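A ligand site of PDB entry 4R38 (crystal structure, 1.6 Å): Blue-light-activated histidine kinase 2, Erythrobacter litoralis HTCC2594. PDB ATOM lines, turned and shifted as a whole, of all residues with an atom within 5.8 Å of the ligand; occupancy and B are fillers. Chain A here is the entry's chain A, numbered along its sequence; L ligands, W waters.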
ATOM      1  N   THR A  27      20.895 -30.565  14.980  1.00  0.00           N
ATOM      2  CA  THR A  27      20.582 -31.755  14.207  1.00  0.00           C
ATOM      3  C   THR A  27      21.834 -32.613  14.092  1.00  0.00           C
ATOM      4  O   THR A  27      22.951 -32.097  14.104  1.00  0.00           O
ATOM      5  CB  THR A  27      20.143 -31.395  12.792  1.00  0.00           C
ATOM      6  OG1 THR A  27      21.213 -30.703  12.126  1.00  0.00           O
ATOM      7  CG2 THR A  27      18.889 -30.518  12.795  1.00  0.00           C
ATOM      8  N   ILE A  28      21.654 -33.931  14.004  1.00  0.00           N
ATOM      9  CA  ILE A  28      22.778 -34.820  13.779  1.00  0.00           C
ATOM     10  C   ILE A  28      22.328 -35.739  12.655  1.00  0.00           C
ATOM     11  O   ILE A  28      21.190 -36.197  12.689  1.00  0.00           O
ATOM     12  CB  ILE A  28      23.108 -35.668  15.020  1.00  0.00           C
ATOM     13  CG1 ILE A  28      23.537 -34.771  16.208  1.00  0.00           C
ATOM     14  CG2 ILE A  28      24.212 -36.693  14.731  1.00  0.00           C
ATOM     15  CD1 ILE A  28      23.620 -35.499  17.511  1.00  0.00           C
ATOM     16  N   ALA A  29      23.209 -35.987  11.688  1.00  0.00           N
ATOM     17  CA  ALA A  29      22.916 -36.873  10.550  1.00  0.00           C
ATOM     18  C   ALA A  29      23.924 -38.001  10.516  1.00  0.00           C
ATOM     19  O   ALA A  29      25.070 -37.796  10.851  1.00  0.00           O
ATOM     20  CB  ALA A  29      22.995 -36.104   9.269  1.00  0.00           C
ATOM     21  N   ILE A  31      25.880 -39.657   8.046  1.00  0.00           N
ATOM     22  CA  ILE A  31      26.236 -39.445   6.641  1.00  0.00           C
ATOM     23  C   ILE A  31      26.842 -40.676   5.983  1.00  0.00           C
ATOM     24  O   ILE A  31      27.191 -40.633   4.807  1.00  0.00           O
ATOM     25  CB  ILE A  31      27.156 -38.201   6.424  1.00  0.00           C
ATOM     26  CG1 ILE A  31      28.518 -38.383   7.072  1.00  0.00           C
ATOM     27  CG2 ILE A  31      26.437 -36.924   6.934  1.00  0.00           C
ATOM     28  CD1 ILE A  31      29.571 -37.443   6.545  1.00  0.00           C
ATOM     29  N   GLU A  36      22.102 -39.614   3.745  1.00  0.00           N
ATOM     30  CA  GLU A  36      22.493 -38.817   4.915  1.00  0.00           C
ATOM     31  C   GLU A  36      21.308 -38.387   5.782  1.00  0.00           C
ATOM     32  O   GLU A  36      21.073 -37.174   5.975  1.00  0.00           O
ATOM     33  CB  GLU A  36      23.226 -37.565   4.456  1.00  0.00           C
ATOM     34  CG  GLU A  36      24.450 -37.820   3.634  1.00  0.00           C
ATOM     35  CD  GLU A  36      24.133 -38.010   2.172  1.00  0.00           C
ATOM     36  OE1 GLU A  36      23.314 -37.212   1.615  1.00  0.00           O
ATOM     37  OE2 GLU A  36      24.681 -38.965   1.578  1.00  0.00           O
ATOM     38  N   LEU A  38      18.739 -37.584   8.809  1.00  0.00           N
ATOM     39  CA  LEU A  38      18.745 -37.103  10.192  1.00  0.00           C
ATOM     40  C   LEU A  38      18.475 -38.258  11.143  1.00  0.00           C
ATOM     41  O   LEU A  38      17.587 -39.059  10.908  1.00  0.00           O
ATOM     42  CB  LEU A  38      17.663 -36.066  10.390  1.00  0.00           C
ATOM     43  CG  LEU A  38      17.914 -34.722   9.738  1.00  0.00           C
ATOM     44  CD1 LEU A  38      16.657 -33.855   9.800  1.00  0.00           C
ATOM     45  CD2 LEU A  38      19.086 -34.006  10.362  1.00  0.00           C
ATOM     46  N   PHE A  45      14.737 -27.186  16.887  1.00  0.00           N
ATOM     47  CA  PHE A  45      14.585 -27.447  15.463  1.00  0.00           C
ATOM     48  C   PHE A  45      13.123 -27.563  15.108  1.00  0.00           C
ATOM     49  O   PHE A  45      12.696 -26.991  14.129  1.00  0.00           O
ATOM     50  CB  PHE A  45      15.290 -28.737  15.078  1.00  0.00           C
ATOM     51  CG  PHE A  45      15.140 -29.104  13.624  1.00  0.00           C
ATOM     52  CD1 PHE A  45      16.076 -28.664  12.695  1.00  0.00           C
ATOM     53  CD2 PHE A  45      14.061 -29.863  13.197  1.00  0.00           C
ATOM     54  CE1 PHE A  45      15.952 -29.014  11.367  1.00  0.00           C
ATOM     55  CE2 PHE A  45      13.937 -30.213  11.869  1.00  0.00           C
ATOM     56  CZ  PHE A  45      14.878 -29.785  10.945  1.00  0.00           C
ATOM     57  N   MET A  48      11.554 -23.988  15.215  1.00  0.00           N
ATOM     58  CA  MET A  48      11.964 -23.170  14.071  1.00  0.00           C
ATOM     59  C   MET A  48      11.341 -23.619  12.751  1.00  0.00           C
ATOM     60  O   MET A  48      10.885 -22.794  11.956  1.00  0.00           O
ATOM     61  CB  MET A  48      13.490 -23.178  13.922  1.00  0.00           C
ATOM     62  CG  MET A  48      14.001 -22.396  12.696  1.00  0.00           C
ATOM     63  SD  MET A  48      15.787 -22.593  12.465  1.00  0.00           S
ATOM     64  CE  MET A  48      15.800 -24.247  11.745  1.00  0.00           C
ATOM     65  N   ASN A  60      16.768 -36.872   4.762  1.00  0.00           N
ATOM     66  CA  ASN A  60      17.771 -35.828   4.532  1.00  0.00           C
ATOM     67  C   ASN A  60      17.186 -34.437   4.782  1.00  0.00           C
ATOM     68  O   ASN A  60      16.081 -34.147   4.347  1.00  0.00           O
ATOM     69  CB  ASN A  60      18.284 -35.898   3.102  1.00  0.00           C
ATOM     70  CG  ASN A  60      19.445 -34.988   2.853  1.00  0.00           C
ATOM     71  OD1 ASN A  60      19.289 -33.759   2.708  1.00  0.00           O
ATOM     72  ND2 ASN A  60      20.625 -35.562   2.753  1.00  0.00           N
ATOM     73  N   CYS A  61      17.932 -33.588   5.475  1.00  0.00           N
ATOM     74  CA  CYS A  61      17.433 -32.268   5.855  1.00  0.00           C
ATOM     75  C   CYS A  61      17.016 -31.359   4.685  1.00  0.00           C
ATOM     76  O   CYS A  61      16.454 -30.284   4.922  1.00  0.00           O
ATOM     77  CB  CYS A  61      18.475 -31.526   6.704  1.00  0.00           C
ATOM     78  SG  CYS A  61      17.736 -30.395   7.928  1.00  0.00           S
ATOM     79  N   ARG A  62      17.272 -31.764   3.426  1.00  0.00           N
ATOM     80  CA  ARG A  62      16.967 -30.880   2.316  1.00  0.00           C
ATOM     81  C   ARG A  62      15.466 -30.705   2.069  1.00  0.00           C
ATOM     82  O   ARG A  62      15.089 -29.923   1.214  1.00  0.00           O
ATOM     83  CB  ARG A  62      17.629 -31.325   0.999  1.00  0.00           C
ATOM     84  CG  ARG A  62      17.095 -32.610   0.409  1.00  0.00           C
ATOM     85  CD  ARG A  62      17.749 -32.903  -0.944  1.00  0.00           C
ATOM     86  NE  ARG A  62      19.206 -33.066  -0.872  1.00  0.00           N
ATOM     87  CZ  ARG A  62      19.826 -34.225  -0.656  1.00  0.00           C
ATOM     88  NH1 ARG A  62      19.134 -35.349  -0.460  1.00  0.00           N
ATOM     89  NH2 ARG A  62      21.160 -34.257  -0.587  1.00  0.00           N
ATOM     90  N   LEU A  64      13.804 -29.038   3.743  1.00  0.00           N
ATOM     91  CA  LEU A  64      13.642 -27.622   4.105  1.00  0.00           C
ATOM     92  C   LEU A  64      13.901 -26.669   2.951  1.00  0.00           C
ATOM     93  O   LEU A  64      13.583 -25.489   3.033  1.00  0.00           O
ATOM     94  CB  LEU A  64      14.591 -27.267   5.257  1.00  0.00           C
ATOM     95  CG  LEU A  64      14.292 -27.853   6.632  1.00  0.00           C
ATOM     96  CD1 LEU A  64      15.407 -27.451   7.589  1.00  0.00           C
ATOM     97  CD2 LEU A  64      12.921 -27.392   7.108  1.00  0.00           C
ATOM     98  N   GLN A  65      14.490 -27.181   1.877  1.00  0.00           N
ATOM     99  CA  GLN A  65      14.855 -26.362   0.734  1.00  0.00           C
ATOM    100  C   GLN A  65      13.706 -26.240  -0.258  1.00  0.00           C
ATOM    101  O   GLN A  65      12.704 -26.957  -0.193  1.00  0.00           O
ATOM    102  CB  GLN A  65      16.095 -26.927   0.026  1.00  0.00           C
ATOM    103  CG  GLN A  65      17.343 -26.829   0.878  1.00  0.00           C
ATOM    104  CD  GLN A  65      18.485 -27.734   0.433  1.00  0.00           C
ATOM    105  OE1 GLN A  65      18.505 -28.253  -0.703  1.00  0.00           O
ATOM    106  NE2 GLN A  65      19.449 -27.903   1.329  1.00  0.00           N
ATOM    107  N   VAL A  74      24.051 -24.929  -1.965  1.00  0.00           N
ATOM    108  CA  VAL A  74      23.767 -26.338  -1.741  1.00  0.00           C
ATOM    109  C   VAL A  74      25.016 -27.156  -2.080  1.00  0.00           C
ATOM    110  O   VAL A  74      25.380 -28.056  -1.335  1.00  0.00           O
ATOM    111  CB  VAL A  74      22.545 -26.818  -2.597  1.00  0.00           C
ATOM    112  CG1 VAL A  74      22.431 -28.341  -2.594  1.00  0.00           C
ATOM    113  CG2 VAL A  74      21.249 -26.210  -2.034  1.00  0.00           C
ATOM    114  N   GLU A  75      25.683 -26.819  -3.176  1.00  0.00           N
ATOM    115  CA  GLU A  75      26.891 -27.579  -3.555  1.00  0.00           C
ATOM    116  C   GLU A  75      28.067 -27.364  -2.582  1.00  0.00           C
ATOM    117  O   GLU A  75      28.851 -28.289  -2.344  1.00  0.00           O
ATOM    118  CB  GLU A  75      27.278 -27.314  -5.017  1.00  0.00           C
ATOM    119  CG  GLU A  75      28.608 -27.922  -5.466  1.00  0.00           C
ATOM    120  CD  GLU A  75      28.801 -29.403  -5.075  1.00  0.00           C
ATOM    121  OE1 GLU A  75      27.801 -30.176  -4.888  1.00  0.00           O
ATOM    122  OE2 GLU A  75      29.974 -29.806  -4.974  1.00  0.00           O
ATOM    123  N   LEU A  77      27.715 -27.034   0.677  1.00  0.00           N
ATOM    124  CA  LEU A  77      27.301 -27.962   1.685  1.00  0.00           C
ATOM    125  C   LEU A  77      27.601 -29.410   1.318  1.00  0.00           C
ATOM    126  O   LEU A  77      28.170 -30.137   2.100  1.00  0.00           O
ATOM    127  CB  LEU A  77      25.825 -27.805   2.007  1.00  0.00           C
ATOM    128  CG  LEU A  77      25.340 -26.478   2.599  1.00  0.00           C
ATOM    129  CD1 LEU A  77      23.832 -26.522   2.862  1.00  0.00           C
ATOM    130  CD2 LEU A  77      26.062 -26.110   3.844  1.00  0.00           C
ATOM    131  N   ALA A  78      27.179 -29.840   0.136  1.00  0.00           N
ATOM    132  CA  ALA A  78      27.452 -31.215  -0.285  1.00  0.00           C
ATOM    133  C   ALA A  78      28.950 -31.487  -0.326  1.00  0.00           C
ATOM    134  O   ALA A  78      29.395 -32.567   0.065  1.00  0.00           O
ATOM    135  CB  ALA A  78      26.835 -31.488  -1.650  1.00  0.00           C
ATOM    136  N   ILE A  81      30.314 -32.131   3.083  1.00  0.00           N
ATOM    137  CA  ILE A  81      29.929 -33.463   3.536  1.00  0.00           C
ATOM    138  C   ILE A  81      30.801 -34.563   2.913  1.00  0.00           C
ATOM    139  O   ILE A  81      31.277 -35.440   3.617  1.00  0.00           O
ATOM    140  CB  ILE A  81      28.435 -33.747   3.291  1.00  0.00           C
ATOM    141  CG1 ILE A  81      27.593 -32.920   4.276  1.00  0.00           C
ATOM    142  CG2 ILE A  81      28.118 -35.235   3.443  1.00  0.00           C
ATOM    143  CD1 ILE A  81      26.138 -32.796   3.875  1.00  0.00           C
ATOM    144  N   ILE A  91      21.303 -20.168   3.869  1.00  0.00           N
ATOM    145  CA  ILE A  91      20.544 -20.841   2.816  1.00  0.00           C
ATOM    146  C   ILE A  91      19.035 -20.575   3.018  1.00  0.00           C
ATOM    147  O   ILE A  91      18.548 -20.478   4.142  1.00  0.00           O
ATOM    148  CB  ILE A  91      20.859 -22.354   2.826  1.00  0.00           C
ATOM    149  CG1 ILE A  91      20.351 -23.042   1.569  1.00  0.00           C
ATOM    150  CG2 ILE A  91      20.335 -23.006   4.133  1.00  0.00           C
ATOM    151  CD1 ILE A  91      20.839 -24.482   1.427  1.00  0.00           C
ATOM    152  N   TYR A  92      18.309 -20.401   1.920  1.00  0.00           N
ATOM    153  CA  TYR A  92      16.874 -20.169   2.007  1.00  0.00           C
ATOM    154  C   TYR A  92      16.113 -21.465   2.212  1.00  0.00           C
ATOM    155  O   TYR A  92      16.246 -22.419   1.439  1.00  0.00           O
ATOM    156  CB  TYR A  92      16.367 -19.460   0.750  1.00  0.00           C
ATOM    157  CG  TYR A  92      15.052 -18.737   0.945  1.00  0.00           C
ATOM    158  CD1 TYR A  92      15.013 -17.471   1.532  1.00  0.00           C
ATOM    159  CD2 TYR A  92      13.842 -19.308   0.566  1.00  0.00           C
ATOM    160  CE1 TYR A  92      13.818 -16.795   1.703  1.00  0.00           C
ATOM    161  CE2 TYR A  92      12.629 -18.643   0.767  1.00  0.00           C
ATOM    162  CZ  TYR A  92      12.630 -17.385   1.317  1.00  0.00           C
ATOM    163  OH  TYR A  92      11.435 -16.717   1.509  1.00  0.00           O
ATOM    164  N   ASN A  93      15.301 -21.491   3.253  1.00  0.00           N
ATOM    165  CA  ASN A  93      14.577 -22.681   3.659  1.00  0.00           C
ATOM    166  C   ASN A  93      13.113 -22.290   3.810  1.00  0.00           C
ATOM    167  O   ASN A  93      12.775 -21.103   3.762  1.00  0.00           O
ATOM    168  CB  ASN A  93      15.074 -23.226   4.995  1.00  0.00           C
ATOM    169  CG  ASN A  93      16.321 -24.152   4.893  1.00  0.00           C
ATOM    170  OD1 ASN A  93      16.782 -24.647   5.920  1.00  0.00           O
ATOM    171  ND2 ASN A  93      16.845 -24.388   3.683  1.00  0.00           N
ATOM    172  N   ASN A 103      18.283 -19.395   6.772  1.00  0.00           N
ATOM    173  CA  ASN A 103      18.804 -20.305   7.764  1.00  0.00           C
ATOM    174  C   ASN A 103      20.316 -20.211   7.686  1.00  0.00           C
ATOM    175  O   ASN A 103      20.914 -20.540   6.664  1.00  0.00           O
ATOM    176  CB  ASN A 103      18.332 -21.721   7.439  1.00  0.00           C
ATOM    177  CG  ASN A 103      18.776 -22.767   8.458  1.00  0.00           C
ATOM    178  OD1 ASN A 103      19.664 -22.541   9.329  1.00  0.00           O
ATOM    179  ND2 ASN A 103      18.168 -23.919   8.380  1.00  0.00           N
ATOM    180  N   LEU A 105      23.309 -21.885   8.646  1.00  0.00           N
ATOM    181  CA  LEU A 105      23.656 -23.236   9.024  1.00  0.00           C
ATOM    182  C   LEU A 105      25.163 -23.324   9.266  1.00  0.00           C
ATOM    183  O   LEU A 105      25.964 -22.834   8.467  1.00  0.00           O
ATOM    184  CB  LEU A 105      23.228 -24.175   7.893  1.00  0.00           C
ATOM    185  CG  LEU A 105      23.540 -25.670   7.971  1.00  0.00           C
ATOM    186  CD1 LEU A 105      22.796 -26.386   9.086  1.00  0.00           C
ATOM    187  CD2 LEU A 105      23.201 -26.314   6.613  1.00  0.00           C
ATOM    188  N   MET A 107      27.791 -26.461  10.197  1.00  0.00           N
ATOM    189  CA  MET A 107      27.857 -27.884  10.439  1.00  0.00           C
ATOM    190  C   MET A 107      29.227 -28.438  10.157  1.00  0.00           C
ATOM    191  O   MET A 107      30.111 -27.763   9.636  1.00  0.00           O
ATOM    192  CB  MET A 107      26.785 -28.599   9.604  1.00  0.00           C
ATOM    193  CG  MET A 107      27.092 -28.582   8.152  1.00  0.00           C
ATOM    194  SD  MET A 107      25.959 -29.539   7.138  1.00  0.00           S
ATOM    195  CE  MET A 107      26.769 -29.512   5.545  1.00  0.00           C
ATOM    196  N   PHE A 120      27.556 -36.138  11.274  1.00  0.00           N
ATOM    197  CA  PHE A 120      27.701 -34.704  11.076  1.00  0.00           C
ATOM    198  C   PHE A 120      26.726 -34.073  12.024  1.00  0.00           C
ATOM    199  O   PHE A 120      25.609 -34.564  12.202  1.00  0.00           O
ATOM    200  CB  PHE A 120      27.370 -34.316   9.637  1.00  0.00           C
ATOM    201  CG  PHE A 120      28.556 -33.824   8.843  1.00  0.00           C
ATOM    202  CD1 PHE A 120      28.548 -32.561   8.279  1.00  0.00           C
ATOM    203  CD2 PHE A 120      29.655 -34.625   8.641  1.00  0.00           C
ATOM    204  CE1 PHE A 120      29.632 -32.106   7.564  1.00  0.00           C
ATOM    205  CE2 PHE A 120      30.756 -34.158   7.920  1.00  0.00           C
ATOM    206  CZ  PHE A 120      30.727 -32.912   7.375  1.00  0.00           C
ATOM    207  N   VAL A 121      27.138 -32.962  12.628  1.00  0.00           N
ATOM    208  CA  VAL A 121      26.266 -32.167  13.472  1.00  0.00           C
ATOM    209  C   VAL A 121      26.152 -30.800  12.863  1.00  0.00           C
ATOM    210  O   VAL A 121      27.113 -30.298  12.257  1.00  0.00           O
ATOM    211  CB  VAL A 121      26.824 -32.040  14.946  1.00  0.00           C
ATOM    212  CG1 VAL A 121      28.193 -31.374  14.972  1.00  0.00           C
ATOM    213  CG2 VAL A 121      25.845 -31.282  15.836  1.00  0.00           C
ATOM    214  N   GLY A 122      24.973 -30.196  12.998  1.00  0.00           N
ATOM    215  CA  GLY A 122      24.694 -28.868  12.476  1.00  0.00           C
ATOM    216  C   GLY A 122      23.829 -28.078  13.447  1.00  0.00           C
ATOM    217  O   GLY A 122      22.985 -28.642  14.157  1.00  0.00           O
ATOM    218  N   GLN A 124      21.285 -24.560  13.385  1.00  0.00           N
ATOM    219  CA  GLN A 124      20.547 -23.680  12.514  1.00  0.00           C
ATOM    220  C   GLN A 124      20.140 -22.450  13.279  1.00  0.00           C
ATOM    221  O   GLN A 124      19.569 -22.554  14.374  1.00  0.00           O
ATOM    222  CB  GLN A 124      19.275 -24.347  12.025  1.00  0.00           C
ATOM    223  CG  GLN A 124      19.520 -25.541  11.171  1.00  0.00           C
ATOM    224  CD  GLN A 124      19.804 -26.816  11.926  1.00  0.00           C
ATOM    225  OE1 GLN A 124      19.530 -26.930  13.118  1.00  0.00           O
ATOM    226  NE2 GLN A 124      20.340 -27.799  11.208  1.00  0.00           N
HETATM  227  N1  LIG L   1      20.128 -28.029   4.614  1.00  0.00           N
HETATM  228  C1  LIG L   1      19.160 -27.093   4.759  1.00  0.00           C
HETATM  229  O1  LIG L   1      18.633 -26.613   3.776  1.00  0.00           O
HETATM  230  N2  LIG L   1      18.791 -26.696   6.017  1.00  0.00           N
HETATM  231  C2  LIG L   1      19.284 -27.275   7.126  1.00  0.00           C
HETATM  232  O2  LIG L   1      18.926 -26.897   8.262  1.00  0.00           O
HETATM  233  C3  LIG L   1      20.261 -28.299   7.016  1.00  0.00           C
HETATM  234  N3  LIG L   1      20.778 -28.958   8.081  1.00  0.00           N
HETATM  235  C4  LIG L   1      21.679 -29.941   7.920  1.00  0.00           C
HETATM  236  C5  LIG L   1      22.254 -30.636   9.023  1.00  0.00           C
HETATM  237  C6  LIG L   1      23.186 -31.655   8.843  1.00  0.00           C
HETATM  238  C7  LIG L   1      23.734 -32.331  10.126  1.00  0.00           C
HETATM  239  C8  LIG L   1      23.585 -31.998   7.553  1.00  0.00           C
HETATM  240  C9  LIG L   1      24.606 -33.095   7.233  1.00  0.00           C
HETATM  241  C10 LIG L   1      23.054 -31.337   6.484  1.00  0.00           C
HETATM  242  C11 LIG L   1      22.096 -30.290   6.617  1.00  0.00           C
HETATM  243  N4  LIG L   1      21.559 -29.675   5.498  1.00  0.00           N
HETATM  244  C12 LIG L   1      20.642 -28.657   5.681  1.00  0.00           C
HETATM  245  C13 LIG L   1      22.017 -29.951   4.140  1.00  0.00           C
HETATM  246  C14 LIG L   1      21.244 -30.990   3.330  1.00  0.00           C
HETATM  247  O3  LIG L   1      20.894 -32.012   4.183  1.00  0.00           O
HETATM  248  C15 LIG L   1      22.123 -31.509   2.201  1.00  0.00           C
HETATM  249  O4  LIG L   1      23.239 -32.178   2.739  1.00  0.00           O
HETATM  250  C16 LIG L   1      22.645 -30.374   1.320  1.00  0.00           C
HETATM  251  O5  LIG L   1      21.578 -29.677   0.730  1.00  0.00           O
HETATM  252  C17 LIG L   1      23.542 -30.915   0.221  1.00  0.00           C
HETATM  253  O6  LIG L   1      22.857 -31.859  -0.566  1.00  0.00           O
HETATM  254  O   HOH W   1      19.927 -30.327  -1.374  1.00  0.00           O
HETATM  255  O   HOH W   2      23.472 -34.573   1.675  1.00  0.00           O
HETATM  256  O   HOH W   3      20.698 -34.393   6.144  1.00  0.00           O
HETATM  257  O   HOH W   4      23.429 -31.564  -3.335  1.00  0.00           O
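Water W2 lies within hydrogen-bond range of an oxygen (O4) of the ligand, the side-chain carboxylate (OE1) of Glu 36, the side-chain amide nitrogen (ND2) of Asn 60 and the guanidinium group (NH2) of Arg 62.
Water W1 lies within hydrogen-bond range of OE1 of Gln 65, O5 of the ligand and NE of Arg 62.
Water W3 lies within hydrogen-bond range of the backbone carbonyl oxygen (O) of Glu 36, the backbone NH (N) of Cys 61 and an oxygen (O3) of the ligand.
OD1 of Asn 93 is in hydrogen-bond range of ND2 of Asn 103.
The backbone carbonyl oxygen of Phe 120 sits at hydrogen-bond distance from the backbone NH of Ala 29, 2.8 Å away.
O of Asn 103 is in hydrogen-bond range of N of Ile 91, 2.8 Å away.
The side-chain hydroxyl (OG1) of Thr 27 sits at hydrogen-bond distance from the side-chain amide nitrogen (NE2) of Gln 124, at 3.2 Å.
N of Thr 27 sits at hydrogen-bond distance from O of Gly 122, at 3.0 Å.
N of Arg 62 lies within hydrogen-bond range of OD1 of Asn 60 (2.9 Å).
The side-chain amide nitrogen (ND2) of Asn 60 lies within hydrogen-bond range of the side-chain carboxylate (OE1) of Glu 36, at 3.4 Å.
O2 of the ligand lies within hydrogen-bond range of ND2 of Asn 103, at 3.1 Å.
OD1 of Asn 60 is in hydrogen-bond range of O3 of the ligand (2.8 Å).
The side-chain amide nitrogen (NE2) of Gln 124 sits at hydrogen-bond distance from a nitrogen (N3) of the ligand (3.4 Å).
O1 of the ligand lies within hydrogen-bond range of ND2 of Asn 93 (2.9 Å).
SG of Cys 61 sits at hydrogen-bond distance from N3 of the ligand.
An oxygen (O5) of the ligand is in hydrogen-bond range of the side-chain amide nitrogen (NE2) of Gln 65, 2.8 Å away.
O6 of the ligand is in hydrogen-bond range of NH2 of Arg 62, 2.9 Å away.
Thr 27 touches the ligand (OG1 to C5, 3.3 Å).
CB of Ala 29 touches C7 of the ligand, at 3.9 Å.
Leu 64 touches the ligand (CD1 to O2, 3.6 Å).
Val 74 touches the ligand (CG1 to O5, 3.7 Å).
N of Ala 78 touches C17 of the ligand (3.8 Å).
Ile 81 touches the ligand.
Ile 91 touches the ligand (CD1 to O1, 3.9 Å).
CD1 of Leu 105 touches N3 of the ligand, 3.4 Å away.
Met 107 touches the ligand.
Phe 120 touches the ligand (O to C7, 3.6 Å).
Val 121 touches the ligand.
Gly 122 touches the ligand (N to C7, 3.8 Å).
Hydrophobic or aromatic side chains that line the ligand: Ala 29, Leu 64, Val 74, Ala 78, Ile 81, Ile 91, Leu 105, Met 107 and Phe 120.
The nearest printed residue that does not touch the ligand is Leu 77 (4.1 Å).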
